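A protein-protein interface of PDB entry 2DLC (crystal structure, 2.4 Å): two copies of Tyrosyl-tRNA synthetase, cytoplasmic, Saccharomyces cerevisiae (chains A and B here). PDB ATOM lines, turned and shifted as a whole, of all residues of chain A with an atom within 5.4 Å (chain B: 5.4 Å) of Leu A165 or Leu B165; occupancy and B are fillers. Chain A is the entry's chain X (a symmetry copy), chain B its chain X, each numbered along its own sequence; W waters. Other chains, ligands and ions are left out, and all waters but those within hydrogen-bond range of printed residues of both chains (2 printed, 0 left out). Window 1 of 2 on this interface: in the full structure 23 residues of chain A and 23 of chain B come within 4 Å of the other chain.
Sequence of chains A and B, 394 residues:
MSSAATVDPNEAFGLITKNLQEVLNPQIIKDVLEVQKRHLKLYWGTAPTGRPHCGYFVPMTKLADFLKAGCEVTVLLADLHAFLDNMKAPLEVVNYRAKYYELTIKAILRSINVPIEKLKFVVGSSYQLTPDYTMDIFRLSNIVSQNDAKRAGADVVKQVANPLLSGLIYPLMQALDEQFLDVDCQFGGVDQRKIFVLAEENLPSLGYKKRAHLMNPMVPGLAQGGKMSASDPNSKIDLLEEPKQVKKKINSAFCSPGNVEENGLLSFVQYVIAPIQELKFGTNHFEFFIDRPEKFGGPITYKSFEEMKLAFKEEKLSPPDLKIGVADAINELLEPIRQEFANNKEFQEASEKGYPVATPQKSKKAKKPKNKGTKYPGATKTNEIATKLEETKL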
ATOM      1  N   SER A 141      20.211  32.446  18.192  1.00  0.00           N
ATOM      2  CA  SER A 141      20.004  31.888  16.849  1.00  0.00           C
ATOM      3  C   SER A 141      18.600  32.195  16.335  1.00  0.00           C
ATOM      4  O   SER A 141      18.337  32.183  15.124  1.00  0.00           O
ATOM      5  CB  SER A 141      20.257  30.375  16.840  1.00  0.00           C
ATOM      6  OG  SER A 141      19.115  29.653  17.269  1.00  0.00           O
ATOM      7  N   VAL A 144      19.208  36.188  15.375  1.00  0.00           N
ATOM      8  CA  VAL A 144      20.184  36.510  14.331  1.00  0.00           C
ATOM      9  C   VAL A 144      19.910  35.738  13.041  1.00  0.00           C
ATOM     10  O   VAL A 144      19.905  34.504  13.023  1.00  0.00           O
ATOM     11  CB  VAL A 144      21.648  36.248  14.789  1.00  0.00           C
ATOM     12  CG1 VAL A 144      22.651  36.613  13.675  1.00  0.00           C
ATOM     13  CG2 VAL A 144      21.972  37.007  16.073  1.00  0.00           C
ATOM     14  N   SER A 145      19.696  36.479  11.961  1.00  0.00           N
ATOM     15  CA  SER A 145      19.521  35.886  10.643  1.00  0.00           C
ATOM     16  C   SER A 145      20.752  35.100  10.187  1.00  0.00           C
ATOM     17  O   SER A 145      21.880  35.372  10.621  1.00  0.00           O
ATOM     18  CB  SER A 145      19.193  36.971   9.620  1.00  0.00           C
ATOM     19  OG  SER A 145      20.375  37.601   9.161  1.00  0.00           O
ATOM     20  N   GLN A 146      20.521  34.134   9.303  1.00  0.00           N
ATOM     21  CA  GLN A 146      21.601  33.410   8.629  1.00  0.00           C
ATOM     22  C   GLN A 146      22.563  34.373   7.916  1.00  0.00           C
ATOM     23  O   GLN A 146      23.779  34.235   8.026  1.00  0.00           O
ATOM     24  CB  GLN A 146      21.023  32.378   7.655  1.00  0.00           C
ATOM     25  CG  GLN A 146      20.160  31.336   8.347  1.00  0.00           C
ATOM     26  CD  GLN A 146      19.351  30.463   7.401  1.00  0.00           C
ATOM     27  OE1 GLN A 146      18.328  29.902   7.803  1.00  0.00           O
ATOM     28  NE2 GLN A 146      19.809  30.327   6.158  1.00  0.00           N
ATOM     29  N   ALA A 149      24.756  36.396  10.644  1.00  0.00           N
ATOM     30  CA  ALA A 149      25.797  35.568  11.242  1.00  0.00           C
ATOM     31  C   ALA A 149      26.949  35.341  10.254  1.00  0.00           C
ATOM     32  O   ALA A 149      28.112  35.291  10.652  1.00  0.00           O
ATOM     33  CB  ALA A 149      25.223  34.242  11.719  1.00  0.00           C
ATOM     34  N   PRO A 163      31.218  26.711   2.886  1.00  0.00           N
ATOM     35  CA  PRO A 163      31.213  27.127   4.298  1.00  0.00           C
ATOM     36  C   PRO A 163      30.414  26.209   5.224  1.00  0.00           C
ATOM     37  O   PRO A 163      29.330  25.734   4.874  1.00  0.00           O
ATOM     38  CB  PRO A 163      30.567  28.518   4.256  1.00  0.00           C
ATOM     39  CG  PRO A 163      30.669  28.954   2.838  1.00  0.00           C
ATOM     40  CD  PRO A 163      30.560  27.707   2.021  1.00  0.00           C
ATOM     41  N   LEU A 164      30.955  25.981   6.414  1.00  0.00           N
ATOM     42  CA  LEU A 164      30.357  25.061   7.369  1.00  0.00           C
ATOM     43  C   LEU A 164      29.492  25.795   8.372  1.00  0.00           C
ATOM     44  O   LEU A 164      29.745  26.969   8.682  1.00  0.00           O
ATOM     45  CB  LEU A 164      31.446  24.254   8.077  1.00  0.00           C
ATOM     46  CG  LEU A 164      32.358  23.460   7.130  1.00  0.00           C
ATOM     47  CD1 LEU A 164      33.659  23.079   7.833  1.00  0.00           C
ATOM     48  CD2 LEU A 164      31.640  22.230   6.547  1.00  0.00           C
ATOM     49  N   LEU A 165      28.471  25.103   8.877  1.00  0.00           N
ATOM     50  CA  LEU A 165      27.552  25.691   9.853  1.00  0.00           C
ATOM     51  C   LEU A 165      28.287  26.242  11.061  1.00  0.00           C
ATOM     52  O   LEU A 165      27.891  27.265  11.605  1.00  0.00           O
ATOM     53  CB  LEU A 165      26.455  24.702  10.287  1.00  0.00           C
ATOM     54  CG  LEU A 165      25.351  25.252  11.213  1.00  0.00           C
ATOM     55  CD1 LEU A 165      24.792  26.587  10.711  1.00  0.00           C
ATOM     56  CD2 LEU A 165      24.217  24.248  11.423  1.00  0.00           C
ATOM     57  N   SER A 166      29.365  25.572  11.464  1.00  0.00           N
ATOM     58  CA  SER A 166      30.200  26.028  12.589  1.00  0.00           C
ATOM     59  C   SER A 166      30.603  27.502  12.490  1.00  0.00           C
ATOM     60  O   SER A 166      30.681  28.193  13.507  1.00  0.00           O
ATOM     61  CB  SER A 166      31.446  25.145  12.739  1.00  0.00           C
ATOM     62  OG  SER A 166      32.131  25.000  11.510  1.00  0.00           O
ATOM     63  N   GLY A 167      30.827  27.975  11.263  1.00  0.00           N
ATOM     64  CA  GLY A 167      31.219  29.354  11.004  1.00  0.00           C
ATOM     65  C   GLY A 167      30.170  30.379  11.395  1.00  0.00           C
ATOM     66  O   GLY A 167      30.504  31.521  11.727  1.00  0.00           O
ATOM     67  N   LEU A 168      28.905  29.959  11.377  1.00  0.00           N
ATOM     68  CA  LEU A 168      27.783  30.816  11.738  1.00  0.00           C
ATOM     69  C   LEU A 168      27.534  30.852  13.251  1.00  0.00           C
ATOM     70  O   LEU A 168      27.029  31.845  13.781  1.00  0.00           O
ATOM     71  CB  LEU A 168      26.524  30.361  11.000  1.00  0.00           C
ATOM     72  CG  LEU A 168      26.186  30.992   9.637  1.00  0.00           C
ATOM     73  CD1 LEU A 168      27.409  31.469   8.851  1.00  0.00           C
ATOM     74  CD2 LEU A 168      25.342  30.046   8.803  1.00  0.00           C
ATOM     75  N   ILE A 169      27.902  29.775  13.939  1.00  0.00           N
ATOM     76  CA  ILE A 169      27.735  29.681  15.389  1.00  0.00           C
ATOM     77  C   ILE A 169      28.829  30.469  16.103  1.00  0.00           C
ATOM     78  O   ILE A 169      28.589  31.129  17.116  1.00  0.00           O
ATOM     79  CB  ILE A 169      27.700  28.189  15.829  1.00  0.00           C
ATOM     80  CG1 ILE A 169      26.474  27.502  15.218  1.00  0.00           C
ATOM     81  CG2 ILE A 169      27.679  28.061  17.350  1.00  0.00           C
ATOM     82  CD1 ILE A 169      26.534  25.994  15.181  1.00  0.00           C
ATOM     83  N   LEU A 172      28.077  34.162  17.250  1.00  0.00           N
ATOM     84  CA  LEU A 172      27.039  34.199  18.291  1.00  0.00           C
ATOM     85  C   LEU A 172      27.661  33.881  19.648  1.00  0.00           C
ATOM     86  O   LEU A 172      27.420  34.573  20.637  1.00  0.00           O
ATOM     87  CB  LEU A 172      25.904  33.197  18.014  1.00  0.00           C
ATOM     88  CG  LEU A 172      24.986  33.202  16.784  1.00  0.00           C
ATOM     89  CD1 LEU A 172      23.553  32.890  17.207  1.00  0.00           C
ATOM     90  CD2 LEU A 172      25.039  34.463  15.933  1.00  0.00           C
ATOM     91  N   SER B 141      28.118  20.508  13.264  1.00  0.00           N
ATOM     92  CA  SER B 141      28.184  21.809  12.583  1.00  0.00           C
ATOM     93  C   SER B 141      29.500  21.967  11.827  1.00  0.00           C
ATOM     94  O   SER B 141      29.615  22.768  10.888  1.00  0.00           O
ATOM     95  CB  SER B 141      28.000  22.958  13.582  1.00  0.00           C
ATOM     96  OG  SER B 141      29.216  23.284  14.232  1.00  0.00           O
ATOM     97  N   VAL B 144      28.602  19.509   8.604  1.00  0.00           N
ATOM     98  CA  VAL B 144      27.494  19.892   7.727  1.00  0.00           C
ATOM     99  C   VAL B 144      27.642  21.325   7.216  1.00  0.00           C
ATOM    100  O   VAL B 144      27.700  22.279   7.997  1.00  0.00           O
ATOM    101  CB  VAL B 144      26.109  19.732   8.419  1.00  0.00           C
ATOM    102  CG1 VAL B 144      24.963  20.126   7.465  1.00  0.00           C
ATOM    103  CG2 VAL B 144      25.910  18.310   8.940  1.00  0.00           C
ATOM    104  N   SER B 145      27.690  21.464   5.897  1.00  0.00           N
ATOM    105  CA  SER B 145      27.730  22.773   5.262  1.00  0.00           C
ATOM    106  C   SER B 145      26.489  23.613   5.574  1.00  0.00           C
ATOM    107  O   SER B 145      25.411  23.075   5.863  1.00  0.00           O
ATOM    108  CB  SER B 145      27.882  22.619   3.752  1.00  0.00           C
ATOM    109  OG  SER B 145      26.626  22.381   3.143  1.00  0.00           O
ATOM    110  N   GLN B 146      26.653  24.930   5.501  1.00  0.00           N
ATOM    111  CA  GLN B 146      25.533  25.869   5.589  1.00  0.00           C
ATOM    112  C   GLN B 146      24.449  25.550   4.547  1.00  0.00           C
ATOM    113  O   GLN B 146      23.263  25.529   4.867  1.00  0.00           O
ATOM    114  CB  GLN B 146      26.033  27.310   5.448  1.00  0.00           C
ATOM    115  CG  GLN B 146      27.020  27.698   6.537  1.00  0.00           C
ATOM    116  CD  GLN B 146      27.746  29.011   6.286  1.00  0.00           C
ATOM    117  OE1 GLN B 146      28.835  29.226   6.827  1.00  0.00           O
ATOM    118  NE2 GLN B 146      27.147  29.895   5.491  1.00  0.00           N
ATOM    119  N   ALA B 149      22.517  22.150   5.571  1.00  0.00           N
ATOM    120  CA  ALA B 149      21.594  22.351   6.683  1.00  0.00           C
ATOM    121  C   ALA B 149      20.341  23.109   6.223  1.00  0.00           C
ATOM    122  O   ALA B 149      19.239  22.839   6.698  1.00  0.00           O
ATOM    123  CB  ALA B 149      22.280  23.082   7.827  1.00  0.00           C
ATOM    124  N   PRO B 163      15.598  34.254   6.736  1.00  0.00           N
ATOM    125  CA  PRO B 163      15.755  33.028   7.535  1.00  0.00           C
ATOM    126  C   PRO B 163      16.701  33.168   8.728  1.00  0.00           C
ATOM    127  O   PRO B 163      17.755  33.805   8.637  1.00  0.00           O
ATOM    128  CB  PRO B 163      16.329  32.021   6.528  1.00  0.00           C
ATOM    129  CG  PRO B 163      16.036  32.596   5.189  1.00  0.00           C
ATOM    130  CD  PRO B 163      16.100  34.080   5.361  1.00  0.00           C
ATOM    131  N   LEU B 164      16.320  32.551   9.839  1.00  0.00           N
ATOM    132  CA  LEU B 164      17.071  32.665  11.081  1.00  0.00           C
ATOM    133  C   LEU B 164      18.017  31.498  11.260  1.00  0.00           C
ATOM    134  O   LEU B 164      17.751  30.390  10.768  1.00  0.00           O
ATOM    135  CB  LEU B 164      16.112  32.777  12.267  1.00  0.00           C
ATOM    136  CG  LEU B 164      15.129  33.953  12.174  1.00  0.00           C
ATOM    137  CD1 LEU B 164      13.940  33.732  13.109  1.00  0.00           C
ATOM    138  CD2 LEU B 164      15.824  35.300  12.439  1.00  0.00           C
ATOM    139  N   LEU B 165      19.122  31.746  11.962  1.00  0.00           N
ATOM    140  CA  LEU B 165      20.125  30.710  12.210  1.00  0.00           C
ATOM    141  C   LEU B 165      19.519  29.478  12.856  1.00  0.00           C
ATOM    142  O   LEU B 165      19.932  28.364  12.560  1.00  0.00           O
ATOM    143  CB  LEU B 165      21.310  31.234  13.040  1.00  0.00           C
ATOM    144  CG  LEU B 165      22.493  30.267  13.251  1.00  0.00           C
ATOM    145  CD1 LEU B 165      22.926  29.596  11.944  1.00  0.00           C
ATOM    146  CD2 LEU B 165      23.688  30.949  13.919  1.00  0.00           C
ATOM    147  N   SER B 166      18.530  29.682  13.723  1.00  0.00           N
ATOM    148  CA  SER B 166      17.818  28.572  14.380  1.00  0.00           C
ATOM    149  C   SER B 166      17.340  27.491  13.405  1.00  0.00           C
ATOM    150  O   SER B 166      17.355  26.306  13.738  1.00  0.00           O
ATOM    151  CB  SER B 166      16.640  29.094  15.214  1.00  0.00           C
ATOM    152  OG  SER B 166      15.818  29.966  14.463  1.00  0.00           O
ATOM    153  N   GLY B 167      16.947  27.911  12.201  1.00  0.00           N
ATOM    154  CA  GLY B 167      16.466  27.007  11.165  1.00  0.00           C
ATOM    155  C   GLY B 167      17.508  26.019  10.673  1.00  0.00           C
ATOM    156  O   GLY B 167      17.166  24.918  10.228  1.00  0.00           O
ATOM    157  N   LEU B 168      18.779  26.408  10.776  1.00  0.00           N
ATOM    158  CA  LEU B 168      19.897  25.572  10.360  1.00  0.00           C
ATOM    159  C   LEU B 168      20.326  24.580  11.449  1.00  0.00           C
ATOM    160  O   LEU B 168      20.847  23.503  11.149  1.00  0.00           O
ATOM    161  CB  LEU B 168      21.075  26.451   9.942  1.00  0.00           C
ATOM    162  CG  LEU B 168      21.217  26.861   8.466  1.00  0.00           C
ATOM    163  CD1 LEU B 168      19.887  26.948   7.714  1.00  0.00           C
ATOM    164  CD2 LEU B 168      21.995  28.159   8.342  1.00  0.00           C
ATOM    165  N   ILE B 169      20.093  24.943  12.708  1.00  0.00           N
ATOM    166  CA  ILE B 169      20.439  24.089  13.843  1.00  0.00           C
ATOM    167  C   ILE B 169      19.406  22.979  14.007  1.00  0.00           C
ATOM    168  O   ILE B 169      19.738  21.833  14.318  1.00  0.00           O
ATOM    169  CB  ILE B 169      20.595  24.946  15.131  1.00  0.00           C
ATOM    170  CG1 ILE B 169      21.766  25.919  14.964  1.00  0.00           C
ATOM    171  CG2 ILE B 169      20.806  24.065  16.360  1.00  0.00           C
ATOM    172  CD1 ILE B 169      21.770  27.092  15.914  1.00  0.00           C
ATOM    173  N   LEU B 172      20.127  19.453  12.404  1.00  0.00           N
ATOM    174  CA  LEU B 172      21.281  18.801  13.039  1.00  0.00           C
ATOM    175  C   LEU B 172      20.843  18.141  14.345  1.00  0.00           C
ATOM    176  O   LEU B 172      21.172  16.987  14.617  1.00  0.00           O
ATOM    177  CB  LEU B 172      22.417  19.794  13.337  1.00  0.00           C
ATOM    178  CG  LEU B 172      23.178  20.624  12.294  1.00  0.00           C
ATOM    179  CD1 LEU B 172      24.664  20.654  12.640  1.00  0.00           C
ATOM    180  CD2 LEU B 172      22.965  20.207  10.845  1.00  0.00           C
HETATM  181  O   HOH W   1      19.101  35.295   6.421  1.00  0.00           O
HETATM  182  O   HOH W   2      27.659  25.963   2.404  1.00  0.00           O
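O of Ser B141 sits at hydrogen-bond distance from N of Leu A165, at 3.3 Å. O of Ser B141 is in hydrogen-bond range of N of Ser A166 (2.9 Å). The backbone carbonyl oxygen (O) of Val B144 sits at hydrogen-bond distance from the backbone NH (N) of Leu A165, at 3.1 Å. The backbone NH of Gln B146 is in hydrogen-bond range of the backbone carbonyl oxygen of Pro A163, at 2.9 Å. The side-chain amide oxygen (OE1) of Gln B146 lies close to the backbone carbonyl oxygen (O) of Leu A164 (3.1 Å). The backbone carbonyl oxygen (O) of Pro B163 is in hydrogen-bond range of the backbone NH (N) of Gln A146, at 2.9 Å. O of Leu B164 sits close to OE1 of Gln A146. The backbone NH (N) of Leu B165 is in hydrogen-bond range of the backbone carbonyl oxygen (O) of Ser A141, 3.3 Å away. The backbone NH (N) of Leu B165 is in hydrogen-bond range of the backbone carbonyl oxygen (O) of Val A144 (3.1 Å). O of Ser A141 is in hydrogen-bond range of N of Ser B166 (2.9 Å).
Among the printed residues, pairs that only touch across the chains: Leu A168 with Gln B146, Gln A146 with Leu B168, Ser A145 with Pro B163, Pro A163 with Ser B145, Leu A168 with Leu B165, Leu A165 with Leu B168, Leu A164 with Ser B141, Ser A141 with Leu B164, Ile A169 with Ser B141, Ser A141 with Ile B169, Leu A165 with Leu B165, Gln A146 with Leu B165, Leu A165 with Gln B146, Leu A172 with Leu B165, Leu A165 with Leu B172, Leu A168 with Leu B168, Val A144 with Leu B164 and Leu A164 with Val B144.
Leu A165 touches just these residues of chain B: Ser B141 (3.3 Å), Val B144 (3.1 Å), Gln B146 (3.8 Å), Leu B165 (3.7 Å), Leu B168 (3.5 Å) and Leu B172 (3.8 Å). Printed residues of chain A within 4 Å of Leu B165: Ser A141, Val A144, Gln A146, Leu A165, Leu A168 and Leu A172. Printed residues of chain A within 4 Å of Ser B145: Pro A163. Of the printed residues of chain B, Leu A164 touches Ser B141 (3.7 Å), Val B144 (3.9 Å) and Gln B146 (3.1 Å). Ala A149 touches none of the printed residues of chain B. The nearest residue of chain A that does not touch Leu B165 is Ser A145 (4.1 Å).
Of the 13 printed residues of chain A, 11 touch a printed residue of chain B. Printed residues of chain A that touch a printed residue of chain B: Ser A141, Val A144, Ser A145, Gln A146, Pro A163, Leu A164, Leu A165, Ser A166, Leu A168, Ile A169 and Leu A172. Along chain A the printed residues that touch a printed residue of chain B span positions 141 to 172. Of the 13 printed residues of chain B, 11 touch a printed residue of chain A.
Ser A141 touches Leu B164, and with the chains exchanged Leu A164 touches Ser B141. Val A144 touches Leu B164, and with the chains exchanged Leu A164 touches Val B144. Ser A145 touches Pro B163, and with the chains exchanged Pro A163 touches Ser B145. Gln A146 touches Leu B165, and with the chains exchanged Leu A165 touches Gln B146. Positions printed for both chains: 141, 144, 145, 146, 149, 163, 164, 165, 166, 167, 168, 169 and 172. Of the 28 pairs that touch across the chains among the printed residues, 28 have their exchanged pair printed and touching as well.
Water W1 bridges the backbone carbonyl oxygen of Pro B163 (3.0 Å) and the backbone NH of Gln A146 (3.4 Å). Water W2 bridges the backbone carbonyl oxygen (O) of Pro A163 (3.0 Å) and the backbone NH (N) of Gln B146 (3.4 Å).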
